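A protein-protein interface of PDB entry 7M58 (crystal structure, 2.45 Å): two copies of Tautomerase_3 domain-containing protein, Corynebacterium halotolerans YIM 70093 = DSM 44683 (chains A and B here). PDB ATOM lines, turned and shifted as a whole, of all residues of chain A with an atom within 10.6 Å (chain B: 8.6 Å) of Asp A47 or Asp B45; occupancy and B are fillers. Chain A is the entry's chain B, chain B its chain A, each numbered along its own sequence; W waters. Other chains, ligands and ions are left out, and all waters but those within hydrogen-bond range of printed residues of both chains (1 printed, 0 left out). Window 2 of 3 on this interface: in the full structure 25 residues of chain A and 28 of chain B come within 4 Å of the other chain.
The side-chain amide nitrogen (NE2) of Gln B14 sits at hydrogen-bond distance from the backbone carbonyl oxygen (O) of Gly A49 (3.1 Å).
OE1 of Glu A57 is in hydrogen-bond range of NE2 of Gln B14 (3.4 Å).
The side-chain carboxylate (OD2) of Asp A47 is in salt-bridge range of the guanidinium group (NH2) of Arg B17 (3.2 Å).
N of Phe B43 is in hydrogen-bond range of O of Ala A50, at 3.0 Å.
The side-chain carboxylate (OD2) of Asp B45 sits close to the side-chain carboxylate (OD2) of Asp A47, 3.3 Å away.
The guanidinium group (NH1) of Arg B17 lies close to the backbone carbonyl oxygen (O) of Gly A49 (3.4 Å).
Among the printed residues, merely in contact across the chains: Leu A46 with Ile B42 (3.7 Å), Leu A46 with Phe B43 (3.7 Å), Leu A46 with Asn B44 (3.7 Å), Ala A50 with Arg B17 (3.6 Å), Ala A50 with Ile B42 (3.4 Å), Leu A51 with Ile B42 (3.9 Å), Phe A52 with Gln B14 (3.6 Å), Phe A52 with Arg B17 (3.8 Å) and Phe A52 with Phe B43 (3.6 Å).
Of chain B, only Arg B17 and Asp B45 come within 4 Å of Asp A47.
Asp B45 touches just one residue of chain A: Asp A47.
No residue of chain B comes within 4 Å of Ala A48.
Ala B9 touches none of the printed residues of chain A.
No residue of chain A comes within 4 Å of Leu B46.
Of the printed residues of chain B, Ala A50 touches Arg B17, Ile B42 and Phe B43.
Printed residues of chain A within 4 Å of Gln B14: Gly A49 (3.1 Å), Phe A52 (3.6 Å) and Glu A57 (3.4 Å).
Of the printed residues of chain B, Gly A49 touches Gln B14 and Arg B17.
Printed residues of chain A within 4 Å of Arg B17: Asp A47 (3.2 Å), Gly A49 (3.4 Å), Ala A50 (3.6 Å) and Phe A52 (3.8 Å).
Ser B6 touches none of the printed residues of chain A.
The nearest residue of chain A that does not touch Asp B45 is Ala A50 (5.9 Å).
Water W1 bridges OE1 of Glu A57 (2.7 Å) and NE2 of Gln B14 (3.2 Å).
Leu A46 touches Asn B44, but with the chains exchanged Asn A44 does not touch Leu B46 (9.0 Å).
Asp A47 touches Asp B45, but with the chains exchanged Asp A45 does not touch Asp B47 (10.8 Å).
Positions printed for both chains: 6, 7, 8, 9, 10, 11, 44, 45, 46, 47, 48, 50 and 51.
NH2 of Arg B17 is in salt-bridge range of OD2 of Asp B45, at 2.4 Å.
The backbone carbonyl oxygen (O) of Ile B42 sits at hydrogen-bond distance from the backbone NH (N) of Val B5, at 2.8 Å.
The backbone carbonyl oxygen (O) of Ser A7 is in hydrogen-bond range of the backbone NH (N) of Leu A46 (2.9 Å).
N of Ser B7 is in hydrogen-bond range of O of Asn B44.
O of Val B5 is in hydrogen-bond range of N of Asn B44, at 2.9 Å.
The side-chain amide oxygen (OE1) of Gln B14 is in hydrogen-bond range of the guanidinium group (NH1) of Arg B17 (3.0 Å).
Of the 20 printed residues of chain B, 6 touch a printed residue of chain A.
Hydrophobic or aromatic side chains of chain A within 4 Å of the printed part of chain B: Leu A46, Ala A50, Leu A51 and Phe A52.
Among the printed residues, Asp or Glu carboxylates within 4 Å of a Lys or Arg side-chain nitrogen of the other chain: Asp A47 with Arg B17.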
ATOM      1  N   SER A   6      19.679  -4.293   6.632  1.00  0.00           N
ATOM      2  CA  SER A   6      19.336  -3.721   7.922  1.00  0.00           C
ATOM      3  C   SER A   6      17.893  -3.259   7.895  1.00  0.00           C
ATOM      4  O   SER A   6      17.481  -2.539   6.975  1.00  0.00           O
ATOM      5  CB  SER A   6      20.249  -2.549   8.281  1.00  0.00           C
ATOM      6  OG  SER A   6      21.567  -2.992   8.568  1.00  0.00           O
ATOM      7  N   SER A   7      17.139  -3.684   8.904  1.00  0.00           N
ATOM      8  CA  SER A   7      15.742  -3.318   9.054  1.00  0.00           C
ATOM      9  C   SER A   7      15.370  -3.440  10.525  1.00  0.00           C
ATOM     10  O   SER A   7      16.006  -4.171  11.292  1.00  0.00           O
ATOM     11  CB  SER A   7      14.832  -4.207   8.204  1.00  0.00           C
ATOM     12  OG  SER A   7      14.982  -5.574   8.573  1.00  0.00           O
ATOM     13  N   ARG A   8      14.342  -2.690  10.905  1.00  0.00           N
ATOM     14  CA  ARG A   8      13.744  -2.843  12.219  1.00  0.00           C
ATOM     15  C   ARG A   8      13.407  -4.310  12.454  1.00  0.00           C
ATOM     16  O   ARG A   8      12.790  -4.959  11.602  1.00  0.00           O
ATOM     17  CB  ARG A   8      12.502  -1.963  12.322  1.00  0.00           C
ATOM     18  CG  ARG A   8      11.739  -2.133  13.595  1.00  0.00           C
ATOM     19  CD  ARG A   8      11.566  -0.809  14.322  1.00  0.00           C
ATOM     20  NE  ARG A   8      10.703  -0.957  15.493  1.00  0.00           N
ATOM     21  CZ  ARG A   8       9.399  -0.692  15.493  1.00  0.00           C
ATOM     22  NH1 ARG A   8       8.802  -0.294  14.371  1.00  0.00           N
ATOM     23  NH2 ARG A   8       8.683  -0.862  16.600  1.00  0.00           N
ATOM     24  N   ALA A   9      13.881  -4.844  13.582  1.00  0.00           N
ATOM     25  CA  ALA A   9      13.564  -6.210  13.985  1.00  0.00           C
ATOM     26  C   ALA A   9      12.073  -6.500  13.867  1.00  0.00           C
ATOM     27  O   ALA A   9      11.234  -5.748  14.368  1.00  0.00           O
ATOM     28  CB  ALA A   9      14.032  -6.457  15.425  1.00  0.00           C
ATOM     29  N   GLY A  10      11.750  -7.597  13.194  1.00  0.00           N
ATOM     30  CA  GLY A  10      10.391  -8.025  13.024  1.00  0.00           C
ATOM     31  C   GLY A  10       9.781  -7.664  11.689  1.00  0.00           C
ATOM     32  O   GLY A  10       8.752  -8.244  11.323  1.00  0.00           O
ATOM     33  N   LEU A  11      10.377  -6.718  10.957  1.00  0.00           N
ATOM     34  CA  LEU A  11       9.826  -6.368   9.651  1.00  0.00           C
ATOM     35  C   LEU A  11       9.997  -7.527   8.677  1.00  0.00           C
ATOM     36  O   LEU A  11       9.117  -7.788   7.849  1.00  0.00           O
ATOM     37  CB  LEU A  11      10.491  -5.108   9.101  1.00  0.00           C
ATOM     38  CG  LEU A  11       9.985  -4.685   7.717  1.00  0.00           C
ATOM     39  CD1 LEU A  11       8.593  -4.071   7.862  1.00  0.00           C
ATOM     40  CD2 LEU A  11      10.953  -3.748   6.982  1.00  0.00           C
ATOM     41  N   ASN A  44      20.922  -7.615   9.650  1.00  0.00           N
ATOM     42  CA  ASN A  44      21.169  -6.788  10.830  1.00  0.00           C
ATOM     43  C   ASN A  44      19.831  -6.218  11.300  1.00  0.00           C
ATOM     44  O   ASN A  44      19.258  -5.349  10.632  1.00  0.00           O
ATOM     45  CB  ASN A  44      22.163  -5.665  10.526  1.00  0.00           C
ATOM     46  CG  ASN A  44      23.563  -6.180  10.205  1.00  0.00           C
ATOM     47  OD1 ASN A  44      24.232  -6.776  11.051  1.00  0.00           O
ATOM     48  ND2 ASN A  44      24.009  -5.953   8.971  1.00  0.00           N
ATOM     49  N   ASP A  45      19.321  -6.728  12.427  1.00  0.00           N
ATOM     50  CA  ASP A  45      18.049  -6.270  12.975  1.00  0.00           C
ATOM     51  C   ASP A  45      18.259  -5.120  13.954  1.00  0.00           C
ATOM     52  O   ASP A  45      19.206  -5.122  14.743  1.00  0.00           O
ATOM     53  CB  ASP A  45      17.322  -7.427  13.647  1.00  0.00           C
ATOM     54  CG  ASP A  45      16.904  -8.493  12.647  1.00  0.00           C
ATOM     55  OD1 ASP A  45      16.302  -8.140  11.592  1.00  0.00           O
ATOM     56  OD2 ASP A  45      17.211  -9.683  12.903  1.00  0.00           O
ATOM     57  N   LEU A  46      17.374  -4.131  13.887  1.00  0.00           N
ATOM     58  CA  LEU A  46      17.545  -2.880  14.610  1.00  0.00           C
ATOM     59  C   LEU A  46      16.480  -2.716  15.694  1.00  0.00           C
ATOM     60  O   LEU A  46      15.376  -3.259  15.591  1.00  0.00           O
ATOM     61  CB  LEU A  46      17.516  -1.695  13.632  1.00  0.00           C
ATOM     62  CG  LEU A  46      18.661  -1.676  12.623  1.00  0.00           C
ATOM     63  CD1 LEU A  46      18.481  -0.601  11.567  1.00  0.00           C
ATOM     64  CD2 LEU A  46      19.980  -1.459  13.355  1.00  0.00           C
ATOM     65  N   ASP A  47      16.835  -1.964  16.740  1.00  0.00           N
ATOM     66  CA  ASP A  47      15.911  -1.611  17.812  1.00  0.00           C
ATOM     67  C   ASP A  47      14.733  -0.808  17.281  1.00  0.00           C
ATOM     68  O   ASP A  47      14.678  -0.417  16.117  1.00  0.00           O
ATOM     69  CB  ASP A  47      16.568  -0.730  18.873  1.00  0.00           C
ATOM     70  CG  ASP A  47      17.937  -1.194  19.268  1.00  0.00           C
ATOM     71  OD1 ASP A  47      18.785  -1.437  18.367  1.00  0.00           O
ATOM     72  OD2 ASP A  47      18.161  -1.286  20.497  1.00  0.00           O
ATOM     73  N   ALA A  48      13.778  -0.562  18.182  1.00  0.00           N
ATOM     74  CA  ALA A  48      12.570   0.169  17.819  1.00  0.00           C
ATOM     75  C   ALA A  48      12.893   1.584  17.341  1.00  0.00           C
ATOM     76  O   ALA A  48      12.342   2.045  16.333  1.00  0.00           O
ATOM     77  CB  ALA A  48      11.609   0.213  18.999  1.00  0.00           C
ATOM     78  N   GLY A  49      13.753   2.303  18.059  1.00  0.00           N
ATOM     79  CA  GLY A  49      13.987   3.678  17.651  1.00  0.00           C
ATOM     80  C   GLY A  49      15.364   3.912  17.059  1.00  0.00           C
ATOM     81  O   GLY A  49      15.943   4.993  17.214  1.00  0.00           O
ATOM     82  N   ALA A  50      15.892   2.920  16.345  1.00  0.00           N
ATOM     83  CA  ALA A  50      17.287   2.945  15.928  1.00  0.00           C
ATOM     84  C   ALA A  50      17.486   3.437  14.497  1.00  0.00           C
ATOM     85  O   ALA A  50      18.632   3.605  14.068  1.00  0.00           O
ATOM     86  CB  ALA A  50      17.907   1.557  16.082  1.00  0.00           C
ATOM     87  N   LEU A  51      16.421   3.700  13.749  1.00  0.00           N
ATOM     88  CA  LEU A  51      16.564   4.084  12.355  1.00  0.00           C
ATOM     89  C   LEU A  51      15.934   5.457  12.158  1.00  0.00           C
ATOM     90  O   LEU A  51      14.786   5.678  12.545  1.00  0.00           O
ATOM     91  CB  LEU A  51      15.932   3.025  11.451  1.00  0.00           C
ATOM     92  CG  LEU A  51      16.595   2.838  10.082  1.00  0.00           C
ATOM     93  CD1 LEU A  51      16.167   1.496   9.495  1.00  0.00           C
ATOM     94  CD2 LEU A  51      16.359   3.986   9.103  1.00  0.00           C
ATOM     95  N   PHE A  52      16.688   6.384  11.594  1.00  0.00           N
ATOM     96  CA  PHE A  52      16.223   7.743  11.357  1.00  0.00           C
ATOM     97  C   PHE A  52      16.388   8.088   9.884  1.00  0.00           C
ATOM     98  O   PHE A  52      17.357   7.670   9.241  1.00  0.00           O
ATOM     99  CB  PHE A  52      16.989   8.760  12.210  1.00  0.00           C
ATOM    100  CG  PHE A  52      16.725   8.647  13.682  1.00  0.00           C
ATOM    101  CD1 PHE A  52      17.280   7.616  14.423  1.00  0.00           C
ATOM    102  CD2 PHE A  52      15.948   9.598  14.334  1.00  0.00           C
ATOM    103  CE1 PHE A  52      17.043   7.510  15.783  1.00  0.00           C
ATOM    104  CE2 PHE A  52      15.712   9.505  15.714  1.00  0.00           C
ATOM    105  CZ  PHE A  52      16.263   8.460  16.435  1.00  0.00           C
ATOM    106  N   GLU A  57      12.552   9.813  13.046  1.00  0.00           N
ATOM    107  CA  GLU A  57      12.384   8.366  13.060  1.00  0.00           C
ATOM    108  C   GLU A  57      11.768   7.877  11.757  1.00  0.00           C
ATOM    109  O   GLU A  57      10.794   8.449  11.256  1.00  0.00           O
ATOM    110  CB  GLU A  57      11.506   7.941  14.229  1.00  0.00           C
ATOM    111  CG  GLU A  57      12.168   8.172  15.556  1.00  0.00           C
ATOM    112  CD  GLU A  57      11.800   7.120  16.551  1.00  0.00           C
ATOM    113  OE1 GLU A  57      11.845   7.427  17.761  1.00  0.00           O
ATOM    114  OE2 GLU A  57      11.477   5.993  16.111  1.00  0.00           O
ATOM    115  N   ALA A  58      12.342   6.809  11.219  1.00  0.00           N
ATOM    116  CA  ALA A  58      11.894   6.239   9.968  1.00  0.00           C
ATOM    117  C   ALA A  58      10.557   5.535  10.155  1.00  0.00           C
ATOM    118  O   ALA A  58      10.213   5.119  11.266  1.00  0.00           O
ATOM    119  CB  ALA A  58      12.935   5.249   9.450  1.00  0.00           C
ATOM    120  N   PRO A  59       9.788   5.367   9.085  1.00  0.00           N
ATOM    121  CA  PRO A  59       8.665   4.433   9.150  1.00  0.00           C
ATOM    122  C   PRO A  59       9.197   3.025   9.328  1.00  0.00           C
ATOM    123  O   PRO A  59      10.346   2.724   9.005  1.00  0.00           O
ATOM    124  CB  PRO A  59       7.959   4.614   7.798  1.00  0.00           C
ATOM    125  CG  PRO A  59       9.002   5.147   6.879  1.00  0.00           C
ATOM    126  CD  PRO A  59       9.897   6.008   7.758  1.00  0.00           C
ATOM    127  N   GLU A  60       8.361   2.160   9.898  1.00  0.00           N
ATOM    128  CA  GLU A  60       8.783   0.776  10.104  1.00  0.00           C
ATOM    129  C   GLU A  60       9.171   0.109   8.787  1.00  0.00           C
ATOM    130  O   GLU A  60      10.176  -0.607   8.716  1.00  0.00           O
ATOM    131  CB  GLU A  60       7.673  -0.021  10.791  1.00  0.00           C
ATOM    132  CG  GLU A  60       7.719  -1.515  10.471  1.00  0.00           C
ATOM    133  CD  GLU A  60       7.167  -2.378  11.585  1.00  0.00           C
ATOM    134  OE1 GLU A  60       6.660  -1.808  12.581  1.00  0.00           O
ATOM    135  OE2 GLU A  60       7.228  -3.624  11.457  1.00  0.00           O
ATOM    136  N   GLY A  61       8.404   0.362   7.726  1.00  0.00           N
ATOM    137  CA  GLY A  61       8.642  -0.279   6.451  1.00  0.00           C
ATOM    138  C   GLY A  61       9.792   0.331   5.690  1.00  0.00           C
ATOM    139  O   GLY A  61       9.609   0.923   4.626  1.00  0.00           O
ATOM    140  N   HIS A  62      10.991   0.216   6.244  1.00  0.00           N
ATOM    141  CA  HIS A  62      12.182   0.719   5.581  1.00  0.00           C
ATOM    142  C   HIS A  62      13.298  -0.307   5.721  1.00  0.00           C
ATOM    143  O   HIS A  62      13.514  -0.850   6.809  1.00  0.00           O
ATOM    144  CB  HIS A  62      12.565   2.083   6.169  1.00  0.00           C
ATOM    145  CG  HIS A  62      13.734   2.720   5.510  1.00  0.00           C
ATOM    146  ND1 HIS A  62      13.627   3.427   4.331  1.00  0.00           N
ATOM    147  CD2 HIS A  62      15.032   2.800   5.883  1.00  0.00           C
ATOM    148  CE1 HIS A  62      14.819   3.881   3.983  1.00  0.00           C
ATOM    149  NE2 HIS A  62      15.687   3.522   4.914  1.00  0.00           N
ATOM    150  N   VAL B   5      26.117   4.341  13.483  1.00  0.00           N
ATOM    151  CA  VAL B   5      26.706   4.762  14.750  1.00  0.00           C
ATOM    152  C   VAL B   5      26.765   3.537  15.636  1.00  0.00           C
ATOM    153  O   VAL B   5      25.725   2.961  15.969  1.00  0.00           O
ATOM    154  CB  VAL B   5      25.891   5.873  15.429  1.00  0.00           C
ATOM    155  CG1 VAL B   5      26.488   6.186  16.780  1.00  0.00           C
ATOM    156  CG2 VAL B   5      25.779   7.125  14.532  1.00  0.00           C
ATOM    157  N   SER B   6      27.968   3.129  16.008  1.00  0.00           N
ATOM    158  CA  SER B   6      28.158   1.945  16.828  1.00  0.00           C
ATOM    159  C   SER B   6      28.599   2.362  18.218  1.00  0.00           C
ATOM    160  O   SER B   6      29.547   3.150  18.356  1.00  0.00           O
ATOM    161  CB  SER B   6      29.204   1.012  16.213  1.00  0.00           C
ATOM    162  OG  SER B   6      28.713   0.447  15.016  1.00  0.00           O
ATOM    163  N   SER B   7      27.907   1.838  19.231  1.00  0.00           N
ATOM    164  CA  SER B   7      28.207   2.102  20.632  1.00  0.00           C
ATOM    165  C   SER B   7      27.616   0.978  21.468  1.00  0.00           C
ATOM    166  O   SER B   7      26.692   0.283  21.033  1.00  0.00           O
ATOM    167  CB  SER B   7      27.643   3.443  21.100  1.00  0.00           C
ATOM    168  OG  SER B   7      26.232   3.480  20.964  1.00  0.00           O
ATOM    169  N   ARG B   8      28.175   0.804  22.670  1.00  0.00           N
ATOM    170  CA  ARG B   8      27.604  -0.105  23.662  1.00  0.00           C
ATOM    171  C   ARG B   8      26.122   0.171  23.855  1.00  0.00           C
ATOM    172  O   ARG B   8      25.721   1.311  24.099  1.00  0.00           O
ATOM    173  CB  ARG B   8      28.339   0.057  24.992  1.00  0.00           C
ATOM    174  CG  ARG B   8      27.680  -0.651  26.157  1.00  0.00           C
ATOM    175  CD  ARG B   8      28.128  -2.078  26.332  1.00  0.00           C
ATOM    176  NE  ARG B   8      28.093  -2.469  27.746  1.00  0.00           N
ATOM    177  CZ  ARG B   8      27.008  -2.938  28.363  1.00  0.00           C
ATOM    178  NH1 ARG B   8      25.872  -3.097  27.683  1.00  0.00           N
ATOM    179  NH2 ARG B   8      27.065  -3.266  29.651  1.00  0.00           N
ATOM    180  N   ALA B   9      25.305  -0.866  23.699  1.00  0.00           N
ATOM    181  CA  ALA B   9      23.886  -0.738  24.001  1.00  0.00           C
ATOM    182  C   ALA B   9      23.708  -0.093  25.367  1.00  0.00           C
ATOM    183  O   ALA B   9      24.280  -0.545  26.367  1.00  0.00           O
ATOM    184  CB  ALA B   9      23.201  -2.102  23.963  1.00  0.00           C
ATOM    185  N   GLY B  10      22.903   0.962  25.403  1.00  0.00           N
ATOM    186  CA  GLY B  10      22.673   1.725  26.601  1.00  0.00           C
ATOM    187  C   GLY B  10      23.445   3.023  26.670  1.00  0.00           C
ATOM    188  O   GLY B  10      23.074   3.905  27.449  1.00  0.00           O
ATOM    189  N   LEU B  11      24.488   3.181  25.857  1.00  0.00           N
ATOM    190  CA  LEU B  11      25.242   4.430  25.913  1.00  0.00           C
ATOM    191  C   LEU B  11      24.426   5.595  25.383  1.00  0.00           C
ATOM    192  O   LEU B  11      24.493   6.701  25.928  1.00  0.00           O
ATOM    193  CB  LEU B  11      26.557   4.315  25.147  1.00  0.00           C
ATOM    194  CG  LEU B  11      27.338   5.629  25.061  1.00  0.00           C
ATOM    195  CD1 LEU B  11      27.892   5.991  26.444  1.00  0.00           C
ATOM    196  CD2 LEU B  11      28.470   5.499  24.044  1.00  0.00           C
ATOM    197  N   ILE B  12      23.665   5.385  24.320  1.00  0.00           N
ATOM    198  CA  ILE B  12      22.902   6.459  23.711  1.00  0.00           C
ATOM    199  C   ILE B  12      21.423   6.187  23.957  1.00  0.00           C
ATOM    200  O   ILE B  12      20.829   5.334  23.286  1.00  0.00           O
ATOM    201  CB  ILE B  12      23.212   6.596  22.218  1.00  0.00           C
ATOM    202  CG1 ILE B  12      24.739   6.596  22.025  1.00  0.00           C
ATOM    203  CG2 ILE B  12      22.578   7.880  21.674  1.00  0.00           C
ATOM    204  CD1 ILE B  12      25.261   6.736  20.577  1.00  0.00           C
ATOM    205  N   ASP B  13      20.856   6.888  24.955  1.00  0.00           N
ATOM    206  CA  ASP B  13      19.422   7.166  25.134  1.00  0.00           C
ATOM    207  C   ASP B  13      18.616   7.163  23.851  1.00  0.00           C
ATOM    208  O   ASP B  13      19.140   7.500  22.789  1.00  0.00           O
ATOM    209  CB  ASP B  13      19.228   8.580  25.700  1.00  0.00           C
ATOM    210  CG  ASP B  13      18.979   8.604  27.152  1.00  0.00           C
ATOM    211  OD1 ASP B  13      18.789   7.525  27.731  1.00  0.00           O
ATOM    212  OD2 ASP B  13      19.009   9.720  27.720  1.00  0.00           O
ATOM    213  N   GLN B  14      17.317   6.901  23.938  1.00  0.00           N
ATOM    214  CA  GLN B  14      16.480   7.192  22.782  1.00  0.00           C
ATOM    215  C   GLN B  14      16.421   8.692  22.488  1.00  0.00           C
ATOM    216  O   GLN B  14      16.379   9.094  21.316  1.00  0.00           O
ATOM    217  CB  GLN B  14      15.082   6.615  22.959  1.00  0.00           C
ATOM    218  CG  GLN B  14      14.216   6.827  21.734  1.00  0.00           C
ATOM    219  CD  GLN B  14      14.818   6.203  20.475  1.00  0.00           C
ATOM    220  OE1 GLN B  14      15.309   5.077  20.492  1.00  0.00           O
ATOM    221  NE2 GLN B  14      14.789   6.944  19.379  1.00  0.00           N
ATOM    222  N   ARG B  17      19.762   9.589  21.023  1.00  0.00           N
ATOM    223  CA  ARG B  17      19.721   9.113  19.638  1.00  0.00           C
ATOM    224  C   ARG B  17      19.007  10.110  18.748  1.00  0.00           C
ATOM    225  O   ARG B  17      19.412  10.334  17.606  1.00  0.00           O
ATOM    226  CB  ARG B  17      19.005   7.755  19.516  1.00  0.00           C
ATOM    227  CG  ARG B  17      19.719   6.513  19.970  1.00  0.00           C
ATOM    228  CD  ARG B  17      18.756   5.351  19.712  1.00  0.00           C
ATOM    229  NE  ARG B  17      19.302   4.016  19.955  1.00  0.00           N
ATOM    230  CZ  ARG B  17      18.583   2.899  19.911  1.00  0.00           C
ATOM    231  NH1 ARG B  17      17.284   2.951  19.640  1.00  0.00           N
ATOM    232  NH2 ARG B  17      19.158   1.728  20.118  1.00  0.00           N
ATOM    233  N   ILE B  42      21.599   5.210  11.404  1.00  0.00           N
ATOM    234  CA  ILE B  42      21.314   3.908  11.984  1.00  0.00           C
ATOM    235  C   ILE B  42      22.167   3.739  13.232  1.00  0.00           C
ATOM    236  O   ILE B  42      23.354   4.082  13.233  1.00  0.00           O
ATOM    237  CB  ILE B  42      21.570   2.780  10.974  1.00  0.00           C
ATOM    238  CG1 ILE B  42      20.498   2.808   9.902  1.00  0.00           C
ATOM    239  CG2 ILE B  42      21.515   1.464  11.659  1.00  0.00           C
ATOM    240  CD1 ILE B  42      20.958   2.173   8.602  1.00  0.00           C
ATOM    241  N   PHE B  43      21.565   3.208  14.292  1.00  0.00           N
ATOM    242  CA  PHE B  43      22.255   2.953  15.548  1.00  0.00           C
ATOM    243  C   PHE B  43      22.412   1.451  15.726  1.00  0.00           C
ATOM    244  O   PHE B  43      21.424   0.742  15.951  1.00  0.00           O
ATOM    245  CB  PHE B  43      21.506   3.575  16.725  1.00  0.00           C
ATOM    246  CG  PHE B  43      21.582   5.056  16.742  1.00  0.00           C
ATOM    247  CD1 PHE B  43      22.701   5.699  17.272  1.00  0.00           C
ATOM    248  CD2 PHE B  43      20.559   5.825  16.196  1.00  0.00           C
ATOM    249  CE1 PHE B  43      22.794   7.084  17.267  1.00  0.00           C
ATOM    250  CE2 PHE B  43      20.643   7.215  16.191  1.00  0.00           C
ATOM    251  CZ  PHE B  43      21.761   7.848  16.726  1.00  0.00           C
ATOM    252  N   ASN B  44      23.657   0.981  15.631  1.00  0.00           N
ATOM    253  CA  ASN B  44      24.013  -0.403  15.927  1.00  0.00           C
ATOM    254  C   ASN B  44      24.470  -0.487  17.380  1.00  0.00           C
ATOM    255  O   ASN B  44      25.582  -0.062  17.724  1.00  0.00           O
ATOM    256  CB  ASN B  44      25.102  -0.900  14.981  1.00  0.00           C
ATOM    257  CG  ASN B  44      24.619  -0.986  13.537  1.00  0.00           C
ATOM    258  OD1 ASN B  44      23.700  -1.747  13.221  1.00  0.00           O
ATOM    259  ND2 ASN B  44      25.241  -0.214  12.653  1.00  0.00           N
ATOM    260  N   ASP B  45      23.626  -1.047  18.236  1.00  0.00           N
ATOM    261  CA  ASP B  45      23.985  -1.177  19.637  1.00  0.00           C
ATOM    262  C   ASP B  45      24.744  -2.477  19.867  1.00  0.00           C
ATOM    263  O   ASP B  45      24.370  -3.537  19.352  1.00  0.00           O
ATOM    264  CB  ASP B  45      22.738  -1.112  20.522  1.00  0.00           C
ATOM    265  CG  ASP B  45      22.119   0.285  20.559  1.00  0.00           C
ATOM    266  OD1 ASP B  45      22.784   1.263  20.127  1.00  0.00           O
ATOM    267  OD2 ASP B  45      20.968   0.407  21.024  1.00  0.00           O
ATOM    268  N   LEU B  46      25.784  -2.397  20.684  1.00  0.00           N
ATOM    269  CA  LEU B  46      26.721  -3.492  20.852  1.00  0.00           C
ATOM    270  C   LEU B  46      26.562  -4.107  22.234  1.00  0.00           C
ATOM    271  O   LEU B  46      26.195  -3.419  23.189  1.00  0.00           O
ATOM    272  CB  LEU B  46      28.158  -2.991  20.673  1.00  0.00           C
ATOM    273  CG  LEU B  46      28.531  -2.426  19.311  1.00  0.00           C
ATOM    274  CD1 LEU B  46      29.931  -1.817  19.359  1.00  0.00           C
ATOM    275  CD2 LEU B  46      28.431  -3.517  18.252  1.00  0.00           C
ATOM    276  N   ASP B  47      26.837  -5.413  22.322  1.00  0.00           N
ATOM    277  CA  ASP B  47      26.860  -6.146  23.586  1.00  0.00           C
ATOM    278  C   ASP B  47      27.979  -5.627  24.502  1.00  0.00           C
ATOM    279  O   ASP B  47      28.852  -4.854  24.090  1.00  0.00           O
ATOM    280  CB  ASP B  47      27.013  -7.646  23.325  1.00  0.00           C
ATOM    281  CG  ASP B  47      26.312  -8.501  24.381  1.00  0.00           C
ATOM    282  OD1 ASP B  47      25.942  -7.958  25.448  1.00  0.00           O
ATOM    283  OD2 ASP B  47      26.126  -9.716  24.145  1.00  0.00           O
ATOM    284  N   ALA B  48      27.972  -6.117  25.747  1.00  0.00           N
ATOM    285  CA  ALA B  48      28.815  -5.550  26.803  1.00  0.00           C
ATOM    286  C   ALA B  48      30.311  -5.624  26.489  1.00  0.00           C
ATOM    287  O   ALA B  48      31.042  -4.638  26.672  1.00  0.00           O
ATOM    288  CB  ALA B  48      28.518  -6.245  28.129  1.00  0.00           C
ATOM    289  N   ALA B  50      31.855  -6.319  23.535  1.00  0.00           N
ATOM    290  CA  ALA B  50      31.961  -6.551  22.106  1.00  0.00           C
ATOM    291  C   ALA B  50      32.877  -5.567  21.402  1.00  0.00           C
ATOM    292  O   ALA B  50      33.174  -5.767  20.212  1.00  0.00           O
ATOM    293  CB  ALA B  50      30.574  -6.495  21.464  1.00  0.00           C
ATOM    294  N   LEU B  51      33.372  -4.550  22.111  1.00  0.00           N
ATOM    295  CA  LEU B  51      34.156  -3.477  21.516  1.00  0.00           C
ATOM    296  C   LEU B  51      35.545  -3.461  22.137  1.00  0.00           C
ATOM    297  O   LEU B  51      35.683  -3.358  23.358  1.00  0.00           O
ATOM    298  CB  LEU B  51      33.473  -2.121  21.720  1.00  0.00           C
ATOM    299  CG  LEU B  51      33.758  -1.042  20.656  1.00  0.00           C
ATOM    300  CD1 LEU B  51      32.741   0.099  20.731  1.00  0.00           C
ATOM    301  CD2 LEU B  51      35.196  -0.500  20.644  1.00  0.00           C
HETATM  302  O   HOH W   1      13.238   9.642  18.472  1.00  0.00           O
